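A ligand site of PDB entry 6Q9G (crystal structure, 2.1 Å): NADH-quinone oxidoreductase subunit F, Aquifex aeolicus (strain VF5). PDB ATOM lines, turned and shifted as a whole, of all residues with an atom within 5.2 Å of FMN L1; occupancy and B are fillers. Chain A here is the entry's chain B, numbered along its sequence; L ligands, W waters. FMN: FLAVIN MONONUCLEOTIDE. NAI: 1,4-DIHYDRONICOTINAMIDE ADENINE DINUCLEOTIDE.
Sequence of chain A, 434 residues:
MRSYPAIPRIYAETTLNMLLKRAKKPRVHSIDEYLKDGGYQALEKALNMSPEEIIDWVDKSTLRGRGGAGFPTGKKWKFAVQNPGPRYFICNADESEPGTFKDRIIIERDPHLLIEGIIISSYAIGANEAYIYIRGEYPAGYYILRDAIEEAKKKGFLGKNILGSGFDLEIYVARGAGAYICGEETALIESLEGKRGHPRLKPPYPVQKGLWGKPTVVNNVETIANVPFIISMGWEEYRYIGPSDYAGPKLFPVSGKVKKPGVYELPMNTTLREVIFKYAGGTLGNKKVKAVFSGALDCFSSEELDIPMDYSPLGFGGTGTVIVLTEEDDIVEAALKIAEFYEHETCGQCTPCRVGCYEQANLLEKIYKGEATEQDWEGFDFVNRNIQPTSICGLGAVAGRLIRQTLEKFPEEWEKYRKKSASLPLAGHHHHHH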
ATOM      1  N   GLY A  65     -19.259 -11.787  -1.365  1.00  0.00           N
ATOM      2  CA  GLY A  65     -18.896 -10.869  -0.273  1.00  0.00           C
ATOM      3  C   GLY A  65     -19.633 -11.221   1.010  1.00  0.00           C
ATOM      4  O   GLY A  65     -20.868 -11.116   1.033  1.00  0.00           O
ATOM      5  N   ARG A  66     -18.883 -11.581   2.042  1.00  0.00           N
ATOM      6  CA  ARG A  66     -19.424 -12.049   3.345  1.00  0.00           C
ATOM      7  C   ARG A  66     -19.783 -10.837   4.227  1.00  0.00           C
ATOM      8  O   ARG A  66     -20.341 -11.044   5.319  1.00  0.00           O
ATOM      9  CB  ARG A  66     -18.402 -12.971   4.020  1.00  0.00           C
ATOM     10  CG  ARG A  66     -18.035 -14.211   3.201  1.00  0.00           C
ATOM     11  CD  ARG A  66     -19.191 -15.158   3.028  1.00  0.00           C
ATOM     12  NE  ARG A  66     -18.799 -16.538   2.716  1.00  0.00           N
ATOM     13  CZ  ARG A  66     -19.006 -17.177   1.561  1.00  0.00           C
ATOM     14  NH1 ARG A  66     -18.647 -18.437   1.443  1.00  0.00           N
ATOM     15  NH2 ARG A  66     -19.595 -16.577   0.537  1.00  0.00           N
ATOM     16  N   GLY A  67     -19.471  -9.624   3.763  1.00  0.00           N
ATOM     17  CA  GLY A  67     -19.787  -8.386   4.492  1.00  0.00           C
ATOM     18  C   GLY A  67     -21.285  -8.125   4.533  1.00  0.00           C
ATOM     19  O   GLY A  67     -21.716  -7.335   5.409  1.00  0.00           O
ATOM     20  N   GLY A  68     -22.040  -8.718   3.589  1.00  0.00           N
ATOM     21  CA  GLY A  68     -23.515  -8.743   3.612  1.00  0.00           C
ATOM     22  C   GLY A  68     -24.164  -8.492   2.256  1.00  0.00           C
ATOM     23  O   GLY A  68     -25.332  -8.881   2.123  1.00  0.00           O
ATOM     24  N   ALA A  69     -23.475  -7.883   1.288  1.00  0.00           N
ATOM     25  CA  ALA A  69     -24.076  -7.534  -0.022  1.00  0.00           C
ATOM     26  C   ALA A  69     -23.963  -8.721  -0.985  1.00  0.00           C
ATOM     27  O   ALA A  69     -24.739  -8.738  -1.945  1.00  0.00           O
ATOM     28  CB  ALA A  69     -23.446  -6.293  -0.612  1.00  0.00           C
ATOM     29  N   GLY A  70     -23.024  -9.642  -0.760  1.00  0.00           N
ATOM     30  CA  GLY A  70     -22.889 -10.883  -1.553  1.00  0.00           C
ATOM     31  C   GLY A  70     -22.297 -10.651  -2.931  1.00  0.00           C
ATOM     32  O   GLY A  70     -22.522 -11.504  -3.793  1.00  0.00           O
ATOM     33  N   PHE A  71     -21.535  -9.576  -3.146  1.00  0.00           N
ATOM     34  CA  PHE A  71     -20.933  -9.280  -4.477  1.00  0.00           C
ATOM     35  C   PHE A  71     -19.836 -10.303  -4.789  1.00  0.00           C
ATOM     36  O   PHE A  71     -19.035 -10.635  -3.915  1.00  0.00           O
ATOM     37  CB  PHE A  71     -20.408  -7.846  -4.533  1.00  0.00           C
ATOM     38  CG  PHE A  71     -20.033  -7.388  -5.917  1.00  0.00           C
ATOM     39  CD1 PHE A  71     -20.996  -6.861  -6.760  1.00  0.00           C
ATOM     40  CD2 PHE A  71     -18.740  -7.527  -6.383  1.00  0.00           C
ATOM     41  CE1 PHE A  71     -20.642  -6.452  -8.043  1.00  0.00           C
ATOM     42  CE2 PHE A  71     -18.390  -7.116  -7.652  1.00  0.00           C
ATOM     43  CZ  PHE A  71     -19.349  -6.572  -8.481  1.00  0.00           C
ATOM     44  N   THR A  73     -16.523 -11.964  -5.428  1.00  0.00           N
ATOM     45  CA  THR A  73     -15.211 -11.470  -4.950  1.00  0.00           C
ATOM     46  C   THR A  73     -14.221 -11.429  -6.123  1.00  0.00           C
ATOM     47  O   THR A  73     -13.561 -10.386  -6.315  1.00  0.00           O
ATOM     48  CB  THR A  73     -14.709 -12.310  -3.770  1.00  0.00           C
ATOM     49  OG1 THR A  73     -15.757 -12.374  -2.805  1.00  0.00           O
ATOM     50  CG2 THR A  73     -13.447 -11.744  -3.164  1.00  0.00           C
ATOM     51  N   LYS A  76     -15.006  -8.550  -8.355  1.00  0.00           N
ATOM     52  CA  LYS A  76     -14.565  -7.254  -7.769  1.00  0.00           C
ATOM     53  C   LYS A  76     -13.088  -7.052  -8.106  1.00  0.00           C
ATOM     54  O   LYS A  76     -12.737  -5.980  -8.614  1.00  0.00           O
ATOM     55  CB  LYS A  76     -14.773  -7.205  -6.261  1.00  0.00           C
ATOM     56  CG  LYS A  76     -14.608  -5.828  -5.645  1.00  0.00           C
ATOM     57  CD  LYS A  76     -14.660  -5.829  -4.133  1.00  0.00           C
ATOM     58  CE  LYS A  76     -16.015  -6.280  -3.597  1.00  0.00           C
ATOM     59  NZ  LYS A  76     -16.119  -6.018  -2.151  1.00  0.00           N
ATOM     60  N   ASN A  92     -12.037  -4.791   5.633  1.00  0.00           N
ATOM     61  CA  ASN A  92     -13.106  -4.116   6.415  1.00  0.00           C
ATOM     62  C   ASN A  92     -13.380  -4.948   7.661  1.00  0.00           C
ATOM     63  O   ASN A  92     -14.033  -6.012   7.543  1.00  0.00           O
ATOM     64  CB  ASN A  92     -14.389  -3.916   5.586  1.00  0.00           C
ATOM     65  CG  ASN A  92     -15.379  -2.991   6.275  1.00  0.00           C
ATOM     66  OD1 ASN A  92     -15.329  -2.845   7.498  1.00  0.00           O
ATOM     67  ND2 ASN A  92     -16.259  -2.362   5.508  1.00  0.00           N
ATOM     68  N   ASP A  94     -14.831  -3.349  10.395  1.00  0.00           N
ATOM     69  CA  ASP A  94     -15.630  -2.343  11.150  1.00  0.00           C
ATOM     70  C   ASP A  94     -16.818  -3.012  11.854  1.00  0.00           C
ATOM     71  O   ASP A  94     -17.337  -2.392  12.783  1.00  0.00           O
ATOM     72  CB  ASP A  94     -16.089  -1.172  10.269  1.00  0.00           C
ATOM     73  CG  ASP A  94     -16.510  -0.009  11.148  1.00  0.00           C
ATOM     74  OD1 ASP A  94     -15.630   0.531  11.850  1.00  0.00           O
ATOM     75  OD2 ASP A  94     -17.728   0.320  11.176  1.00  0.00           O
ATOM     76  N   GLU A  95     -17.188  -4.226  11.437  1.00  0.00           N
ATOM     77  CA  GLU A  95     -18.324  -5.054  11.935  1.00  0.00           C
ATOM     78  C   GLU A  95     -19.094  -4.328  13.044  1.00  0.00           C
ATOM     79  O   GLU A  95     -18.680  -4.407  14.205  1.00  0.00           O
ATOM     80  CB  GLU A  95     -17.777  -6.406  12.423  1.00  0.00           C
ATOM     81  CG  GLU A  95     -18.841  -7.309  13.025  1.00  0.00           C
ATOM     82  CD  GLU A  95     -18.377  -8.737  13.245  1.00  0.00           C
ATOM     83  OE1 GLU A  95     -17.675  -9.001  14.251  1.00  0.00           O
ATOM     84  OE2 GLU A  95     -18.730  -9.603  12.399  1.00  0.00           O
ATOM     85  N   SER A  96     -20.189  -3.659  12.689  1.00  0.00           N
ATOM     86  CA  SER A  96     -21.034  -2.893  13.653  1.00  0.00           C
ATOM     87  C   SER A  96     -22.531  -3.121  13.420  1.00  0.00           C
ATOM     88  O   SER A  96     -23.318  -2.453  14.114  1.00  0.00           O
ATOM     89  CB  SER A  96     -20.683  -1.429  13.612  1.00  0.00           C
ATOM     90  OG  SER A  96     -19.326  -1.236  14.004  1.00  0.00           O
ATOM     91  N   ASP A 103     -17.128 -11.765  12.479  1.00  0.00           N
ATOM     92  CA  ASP A 103     -15.755 -11.385  12.049  1.00  0.00           C
ATOM     93  C   ASP A 103     -14.812 -11.365  13.259  1.00  0.00           C
ATOM     94  O   ASP A 103     -13.620 -11.708  13.088  1.00  0.00           O
ATOM     95  CB  ASP A 103     -15.700 -10.027  11.329  1.00  0.00           C
ATOM     96  CG  ASP A 103     -16.531  -9.925  10.054  1.00  0.00           C
ATOM     97  OD1 ASP A 103     -16.900 -10.982   9.499  1.00  0.00           O
ATOM     98  OD2 ASP A 103     -16.781  -8.790   9.612  1.00  0.00           O
ATOM     99  N   TYR A 180     -20.747   3.575  12.989  1.00  0.00           N
ATOM    100  CA  TYR A 180     -21.302   2.475  12.153  1.00  0.00           C
ATOM    101  C   TYR A 180     -21.043   2.756  10.663  1.00  0.00           C
ATOM    102  O   TYR A 180     -20.768   1.801   9.928  1.00  0.00           O
ATOM    103  CB  TYR A 180     -22.793   2.367  12.421  1.00  0.00           C
ATOM    104  CG  TYR A 180     -23.592   1.491  11.493  1.00  0.00           C
ATOM    105  CD1 TYR A 180     -23.548   0.101  11.568  1.00  0.00           C
ATOM    106  CD2 TYR A 180     -24.503   2.052  10.615  1.00  0.00           C
ATOM    107  CE1 TYR A 180     -24.346  -0.688  10.756  1.00  0.00           C
ATOM    108  CE2 TYR A 180     -25.318   1.277   9.805  1.00  0.00           C
ATOM    109  CZ  TYR A 180     -25.238  -0.103   9.881  1.00  0.00           C
ATOM    110  OH  TYR A 180     -26.054  -0.852   9.082  1.00  0.00           O
ATOM    111  N   ILE A 181     -21.214   4.021  10.271  1.00  0.00           N
ATOM    112  CA  ILE A 181     -21.150   4.474   8.844  1.00  0.00           C
ATOM    113  C   ILE A 181     -19.741   4.242   8.290  1.00  0.00           C
ATOM    114  O   ILE A 181     -19.643   4.057   7.084  1.00  0.00           O
ATOM    115  CB  ILE A 181     -21.581   5.949   8.693  1.00  0.00           C
ATOM    116  CG1 ILE A 181     -21.797   6.322   7.222  1.00  0.00           C
ATOM    117  CG2 ILE A 181     -20.587   6.900   9.346  1.00  0.00           C
ATOM    118  CD1 ILE A 181     -22.749   5.404   6.503  1.00  0.00           C
ATOM    119  N   GLY A 183     -18.023   1.735   8.321  1.00  0.00           N
ATOM    120  CA  GLY A 183     -17.968   0.396   7.716  1.00  0.00           C
ATOM    121  C   GLY A 183     -18.406   0.405   6.264  1.00  0.00           C
ATOM    122  O   GLY A 183     -18.079  -0.560   5.556  1.00  0.00           O
ATOM    123  N   GLU A 184     -19.150   1.433   5.848  1.00  0.00           N
ATOM    124  CA  GLU A 184     -19.479   1.678   4.421  1.00  0.00           C
ATOM    125  C   GLU A 184     -18.138   1.966   3.730  1.00  0.00           C
ATOM    126  O   GLU A 184     -17.379   2.837   4.226  1.00  0.00           O
ATOM    127  CB  GLU A 184     -20.515   2.797   4.279  1.00  0.00           C
ATOM    128  CG  GLU A 184     -21.214   2.818   2.926  1.00  0.00           C
ATOM    129  CD  GLU A 184     -20.473   3.556   1.819  1.00  0.00           C
ATOM    130  OE1 GLU A 184     -19.412   4.160   2.082  1.00  0.00           O
ATOM    131  OE2 GLU A 184     -20.980   3.536   0.675  1.00  0.00           O
ATOM    132  N   GLU A 185     -17.850   1.227   2.664  1.00  0.00           N
ATOM    133  CA  GLU A 185     -16.471   1.140   2.097  1.00  0.00           C
ATOM    134  C   GLU A 185     -15.930   2.543   1.770  1.00  0.00           C
ATOM    135  O   GLU A 185     -14.731   2.780   2.035  1.00  0.00           O
ATOM    136  CB  GLU A 185     -16.458   0.193   0.891  1.00  0.00           C
ATOM    137  CG  GLU A 185     -17.443   0.567  -0.198  1.00  0.00           C
ATOM    138  CD  GLU A 185     -17.324  -0.268  -1.448  1.00  0.00           C
ATOM    139  OE1 GLU A 185     -16.553  -1.273  -1.415  1.00  0.00           O
ATOM    140  OE2 GLU A 185     -17.982   0.073  -2.443  1.00  0.00           O
ATOM    141  N   VAL A 218     -12.046  -3.270  -1.380  1.00  0.00           N
ATOM    142  CA  VAL A 218     -12.509  -3.406   0.027  1.00  0.00           C
ATOM    143  C   VAL A 218     -13.194  -4.759   0.126  1.00  0.00           C
ATOM    144  O   VAL A 218     -14.108  -5.014  -0.690  1.00  0.00           O
ATOM    145  CB  VAL A 218     -13.469  -2.286   0.464  1.00  0.00           C
ATOM    146  CG1 VAL A 218     -13.912  -2.488   1.896  1.00  0.00           C
ATOM    147  CG2 VAL A 218     -12.833  -0.924   0.273  1.00  0.00           C
ATOM    148  N   ASN A 219     -12.764  -5.586   1.084  1.00  0.00           N
ATOM    149  CA  ASN A 219     -13.356  -6.916   1.348  1.00  0.00           C
ATOM    150  C   ASN A 219     -13.553  -7.099   2.850  1.00  0.00           C
ATOM    151  O   ASN A 219     -12.771  -6.574   3.639  1.00  0.00           O
ATOM    152  CB  ASN A 219     -12.535  -8.052   0.742  1.00  0.00           C
ATOM    153  CG  ASN A 219     -12.980  -8.391  -0.665  1.00  0.00           C
ATOM    154  OD1 ASN A 219     -12.142  -8.495  -1.561  1.00  0.00           O
ATOM    155  ND2 ASN A 219     -14.285  -8.532  -0.861  1.00  0.00           N
ATOM    156  N   ASN A 220     -14.598  -7.827   3.192  1.00  0.00           N
ATOM    157  CA  ASN A 220     -14.940  -8.192   4.583  1.00  0.00           C
ATOM    158  C   ASN A 220     -13.936  -9.231   5.104  1.00  0.00           C
ATOM    159  O   ASN A 220     -13.500 -10.105   4.311  1.00  0.00           O
ATOM    160  CB  ASN A 220     -16.398  -8.658   4.651  1.00  0.00           C
ATOM    161  CG  ASN A 220     -16.774  -9.247   5.982  1.00  0.00           C
ATOM    162  OD1 ASN A 220     -16.809 -10.477   6.126  1.00  0.00           O
ATOM    163  ND2 ASN A 220     -17.008  -8.398   6.971  1.00  0.00           N
ATOM    164  N   VAL A 221     -13.621  -9.149   6.395  1.00  0.00           N
ATOM    165  CA  VAL A 221     -12.839 -10.138   7.188  1.00  0.00           C
ATOM    166  C   VAL A 221     -13.186 -11.576   6.768  1.00  0.00           C
ATOM    167  O   VAL A 221     -12.257 -12.320   6.405  1.00  0.00           O
ATOM    168  CB  VAL A 221     -13.098  -9.930   8.697  1.00  0.00           C
ATOM    169  CG1 VAL A 221     -12.557 -11.086   9.537  1.00  0.00           C
ATOM    170  CG2 VAL A 221     -12.527  -8.601   9.194  1.00  0.00           C
ATOM    171  N   THR A 223     -14.801 -12.762   4.177  1.00  0.00           N
ATOM    172  CA  THR A 223     -14.522 -13.005   2.726  1.00  0.00           C
ATOM    173  C   THR A 223     -13.041 -13.384   2.582  1.00  0.00           C
ATOM    174  O   THR A 223     -12.748 -14.468   2.008  1.00  0.00           O
ATOM    175  CB  THR A 223     -14.848 -11.803   1.845  1.00  0.00           C
ATOM    176  OG1 THR A 223     -16.182 -11.387   2.129  1.00  0.00           O
ATOM    177  CG2 THR A 223     -14.714 -12.115   0.359  1.00  0.00           C
ATOM    178  N   CYS A 393     -25.716   6.240   0.031  1.00  0.00           N
ATOM    179  CA  CYS A 393     -25.209   4.950   0.584  1.00  0.00           C
ATOM    180  C   CYS A 393     -26.366   4.074   1.082  1.00  0.00           C
ATOM    181  O   CYS A 393     -27.533   4.532   1.124  1.00  0.00           O
ATOM    182  CB  CYS A 393     -24.138   5.166   1.652  1.00  0.00           C
ATOM    183  SG  CYS A 393     -24.743   5.227   3.357  1.00  0.00           S
ATOM    184  N   GLY A 394     -26.037   2.830   1.414  1.00  0.00           N
ATOM    185  CA  GLY A 394     -27.005   1.780   1.753  1.00  0.00           C
ATOM    186  C   GLY A 394     -27.745   2.046   3.050  1.00  0.00           C
ATOM    187  O   GLY A 394     -28.800   1.430   3.234  1.00  0.00           O
ATOM    188  N   LEU A 395     -27.247   2.920   3.916  1.00  0.00           N
ATOM    189  CA  LEU A 395     -27.881   3.216   5.227  1.00  0.00           C
ATOM    190  C   LEU A 395     -29.261   3.862   4.991  1.00  0.00           C
ATOM    191  O   LEU A 395     -30.267   3.305   5.457  1.00  0.00           O
ATOM    192  CB  LEU A 395     -26.964   4.116   6.064  1.00  0.00           C
ATOM    193  CG  LEU A 395     -27.350   4.241   7.537  1.00  0.00           C
ATOM    194  CD1 LEU A 395     -26.123   4.525   8.394  1.00  0.00           C
ATOM    195  CD2 LEU A 395     -28.417   5.303   7.735  1.00  0.00           C
HETATM  196  N1  FMN L   1     -19.008  -4.327   5.313  1.00  0.00           N
HETATM  197  C2  FMN L   1     -18.175  -4.917   6.212  1.00  0.00           C
HETATM  198  O2  FMN L   1     -17.407  -5.818   5.885  1.00  0.00           O
HETATM  199  N3  FMN L   1     -18.138  -4.464   7.512  1.00  0.00           N
HETATM  200  C4  FMN L   1     -18.872  -3.416   8.030  1.00  0.00           C
HETATM  201  O4  FMN L   1     -18.795  -3.143   9.218  1.00  0.00           O
HETATM  202  C4A FMN L   1     -19.734  -2.756   7.045  1.00  0.00           C
HETATM  203  N5  FMN L   1     -20.417  -1.710   7.422  1.00  0.00           N
HETATM  204  C5A FMN L   1     -21.251  -1.106   6.479  1.00  0.00           C
HETATM  205  C6  FMN L   1     -22.028  -0.007   6.865  1.00  0.00           C
HETATM  206  C7  FMN L   1     -22.929   0.582   5.980  1.00  0.00           C
HETATM  207  C7M FMN L   1     -23.754   1.764   6.435  1.00  0.00           C
HETATM  208  C8  FMN L   1     -23.053   0.078   4.679  1.00  0.00           C
HETATM  209  C8M FMN L   1     -24.081   0.634   3.716  1.00  0.00           C
HETATM  210  C9  FMN L   1     -22.251  -0.987   4.273  1.00  0.00           C
HETATM  211  C9A FMN L   1     -21.356  -1.592   5.158  1.00  0.00           C
HETATM  212  N10 FMN L   1     -20.555  -2.708   4.793  1.00  0.00           N
HETATM  213  C10 FMN L   1     -19.748  -3.307   5.723  1.00  0.00           C
HETATM  214  C1' FMN L   1     -20.488  -3.199   3.419  1.00  0.00           C
HETATM  215  C2' FMN L   1     -19.334  -2.566   2.651  1.00  0.00           C
HETATM  216  O2' FMN L   1     -19.751  -1.302   2.115  1.00  0.00           O
HETATM  217  C3' FMN L   1     -18.835  -3.465   1.533  1.00  0.00           C
HETATM  218  O3' FMN L   1     -19.935  -3.948   0.767  1.00  0.00           O
HETATM  219  C4' FMN L   1     -18.018  -4.680   1.976  1.00  0.00           C
HETATM  220  O4' FMN L   1     -17.148  -4.352   3.066  1.00  0.00           O
HETATM  221  C5' FMN L   1     -17.222  -5.248   0.815  1.00  0.00           C
HETATM  222  O5' FMN L   1     -16.708  -6.541   1.187  1.00  0.00           O
HETATM  223  P   FMN L   1     -17.373  -7.936   0.740  1.00  0.00           P
HETATM  224  O1P FMN L   1     -18.673  -8.255   1.451  1.00  0.00           O
HETATM  225  O2P FMN L   1     -17.549  -7.869  -0.773  1.00  0.00           O
HETATM  226  O3P FMN L   1     -16.258  -8.940   1.029  1.00  0.00           O
HETATM  227  PA  NAI L   2     -23.400  -2.937  -2.651  1.00  0.00           P
HETATM  228  O1A NAI L   2     -24.230  -4.072  -3.139  1.00  0.00           O
HETATM  229  O2A NAI L   2     -23.710  -1.592  -3.214  1.00  0.00           O
HETATM  230  O5B NAI L   2     -21.811  -3.198  -2.919  1.00  0.00           O
HETATM  231  C5B NAI L   2     -21.173  -4.449  -2.537  1.00  0.00           C
HETATM  232  C4B NAI L   2     -19.723  -4.473  -2.962  1.00  0.00           C
HETATM  233  O4B NAI L   2     -19.641  -4.707  -4.386  1.00  0.00           O
HETATM  234  C3B NAI L   2     -18.922  -3.205  -2.697  1.00  0.00           C
HETATM  235  O3B NAI L   2     -17.563  -3.522  -2.416  1.00  0.00           O
HETATM  236  C2B NAI L   2     -19.066  -2.449  -4.026  1.00  0.00           C
HETATM  237  O2B NAI L   2     -17.970  -1.567  -4.291  1.00  0.00           O
HETATM  238  C1B NAI L   2     -19.054  -3.598  -5.031  1.00  0.00           C
HETATM  239  N9A NAI L   2     -19.783  -3.307  -6.264  1.00  0.00           N
HETATM  240  C8A NAI L   2     -21.138  -3.238  -6.448  1.00  0.00           C
HETATM  241  N7A NAI L   2     -21.506  -2.933  -7.671  1.00  0.00           N
HETATM  242  C5A NAI L   2     -20.303  -2.793  -8.344  1.00  0.00           C
HETATM  243  C6A NAI L   2     -19.994  -2.433  -9.676  1.00  0.00           C
HETATM  244  N6A NAI L   2     -20.914  -2.138 -10.604  1.00  0.00           N
HETATM  245  N1A NAI L   2     -18.699  -2.354 -10.023  1.00  0.00           N
HETATM  246  C2A NAI L   2     -17.765  -2.617  -9.095  1.00  0.00           C
HETATM  247  N3A NAI L   2     -17.931  -2.963  -7.811  1.00  0.00           N
HETATM  248  C4A NAI L   2     -19.234  -3.020  -7.497  1.00  0.00           C
HETATM  249  O3  NAI L   2     -23.534  -2.826  -1.067  1.00  0.00           O
HETATM  250  PN  NAI L   2     -22.927  -1.888   0.059  1.00  0.00           P
HETATM  251  O1N NAI L   2     -23.743  -0.582   0.059  1.00  0.00           O
HETATM  252  O2N NAI L   2     -21.447  -1.733  -0.026  1.00  0.00           O
HETATM  253  O5D NAI L   2     -23.345  -2.722   1.359  1.00  0.00           O
HETATM  254  C5D NAI L   2     -24.672  -3.009   1.864  1.00  0.00           C
HETATM  255  C4D NAI L   2     -24.554  -4.179   2.803  1.00  0.00           C
HETATM  256  O4D NAI L   2     -23.761  -3.812   3.953  1.00  0.00           O
HETATM  257  C3D NAI L   2     -25.875  -4.708   3.376  1.00  0.00           C
HETATM  258  O3D NAI L   2     -26.321  -5.856   2.673  1.00  0.00           O
HETATM  259  C2D NAI L   2     -25.537  -5.070   4.838  1.00  0.00           C
HETATM  260  O2D NAI L   2     -25.758  -6.448   5.076  1.00  0.00           O
HETATM  261  C1D NAI L   2     -24.039  -4.792   4.928  1.00  0.00           C
HETATM  262  N1N NAI L   2     -23.585  -4.305   6.235  1.00  0.00           N
HETATM  263  C2N NAI L   2     -22.740  -5.095   7.060  1.00  0.00           C
HETATM  264  C3N NAI L   2     -22.310  -4.703   8.268  1.00  0.00           C
HETATM  265  C7N NAI L   2     -21.433  -5.614   9.054  1.00  0.00           C
HETATM  266  O7N NAI L   2     -21.195  -5.354  10.237  1.00  0.00           O
HETATM  267  N7N NAI L   2     -20.932  -6.687   8.462  1.00  0.00           N
HETATM  268  C4N NAI L   2     -22.722  -3.366   8.805  1.00  0.00           C
HETATM  269  C5N NAI L   2     -23.582  -2.613   7.856  1.00  0.00           C
HETATM  270  C6N NAI L   2     -23.970  -3.079   6.679  1.00  0.00           C
HETATM  271  O   HOH W   1     -20.339  -7.771  -1.214  1.00  0.00           O
HETATM  272  O   HOH W   2     -16.395  -6.194   9.204  1.00  0.00           O
HETATM  273  O   HOH W   3     -19.946  -0.838  10.396  1.00  0.00           O
HETATM  274  O   HOH W   4     -20.824  -6.648   1.192  1.00  0.00           O
HETATM  275  O   HOH W   5     -16.816  -9.694  -2.545  1.00  0.00           O
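Water W5 lies within hydrogen-bond range of O2P of FMN L1 (2.6 Å), O of Phe 71 (2.8 Å), OG1 of Thr 73 (2.9 Å), ND2 of Asn 219 (3.3 Å) and N of Gly 65 (3.4 Å). Water W4 lies within hydrogen-bond range of O1P of FMN L1 (2.7 Å), N of Ala 69 (2.9 Å) and N of Gly 68 (3.4 Å). Water W1 lies within hydrogen-bond range of an oxygen (O2P) of FMN L1 (2.8 Å), the backbone NH of Phe 71 (2.9 Å) and the backbone NH of Gly 70 (3.3 Å).
N of Arg 66 is in hydrogen-bond range of OG1 of Thr 223. The side-chain carboxylate (OD2) of Asp 103 is in hydrogen-bond range of the side-chain amide nitrogen (ND2) of Asn 220 (2.7 Å). The backbone NH of Asp 103 is in hydrogen-bond range of the side-chain carboxylate of Glu 95 (2.7 Å). N of Gly 65 lies within hydrogen-bond range of O of Phe 71. O of Gly 65 is in hydrogen-bond range of N of Gly 70 (3.2 Å). The backbone NH of Asp 94 lies within hydrogen-bond range of the side-chain amide oxygen of Asn 92 (3.0 Å). O of Asn 92 sits at hydrogen-bond distance from N of Val 221 (3.4 Å). OG of Ser 96 is in hydrogen-bond range of O of Asp 94, 2.6 Å away.
A nitrogen (N5) of FMN L1 lies close to the backbone carbonyl oxygen (O) of Gly 183. CA of Gly 65 touches O1P of FMN L1, at 3.1 Å. Asp 94 touches FMN L1 (C to O4, 3.3 Å). Ser 96 touches FMN L1 (N to O4, 3.8 Å). Tyr 180 touches FMN L1. Ile 181 touches FMN L1 (CD1 to C7M, 3.8 Å). N of Glu 184 touches C5A of FMN L1 (3.4 Å). Val 218 touches FMN L1 (O to C5', 3.5 Å). Gly 394 touches FMN L1 (CA to C8M, 3.7 Å). Leu 395 touches FMN L1. Hydrophobic or aromatic side chains within 4 Å of FMN L1: Tyr 180, Ile 181, Val 218 and Leu 395. The nearest printed residue that does not touch FMN L1 is Gly 68 (4.02 Å).
OG1 of Thr 223 lies within hydrogen-bond range of O3P of FMN L1 (2.7 Å). O2P of FMN L1 lies within salt-bridge range of NZ of Lys 76 (2.7 Å). ND2 of Asn 219 lies within hydrogen-bond range of O3P of FMN L1, 2.8 Å away. N of Gly 67 lies within hydrogen-bond range of O1P of FMN L1 (2.8 Å). N of Asn 220 lies within hydrogen-bond range of O3P of FMN L1. The side-chain amide nitrogen of Asn 220 is in hydrogen-bond range of an oxygen (O2) of FMN L1 (2.8 Å). The backbone NH (N) of Glu 95 is in hydrogen-bond range of an oxygen (O4) of FMN L1 (2.9 Å). The backbone NH (N) of Glu 185 sits at hydrogen-bond distance from an oxygen (O2') of FMN L1. OD1 of Asn 92 is in hydrogen-bond range of N3 of FMN L1, at 3.2 Å. N of Arg 66 lies within hydrogen-bond range of O1P of FMN L1 (3.4 Å). An oxygen (O3B) of NAI L2 sits at hydrogen-bond distance from the side-chain amino group (NZ) of Lys 76 (2.9 Å). O of Gly 67 lies close to N7N of NAI L2, 3.2 Å away. The side-chain carboxylate of Glu 185 sits at hydrogen-bond distance from an oxygen (O2B) of NAI L2 (2.5 Å). An oxygen (O7N) of NAI L2 sits at hydrogen-bond distance from the backbone NH (N) of Ser 96. O3D of NAI L2 is in hydrogen-bond range of O of Gly 68, at 3.2 Å.
An oxygen (O2N) of NAI L2 sits at hydrogen-bond distance from an oxygen (O2') of FMN L1.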
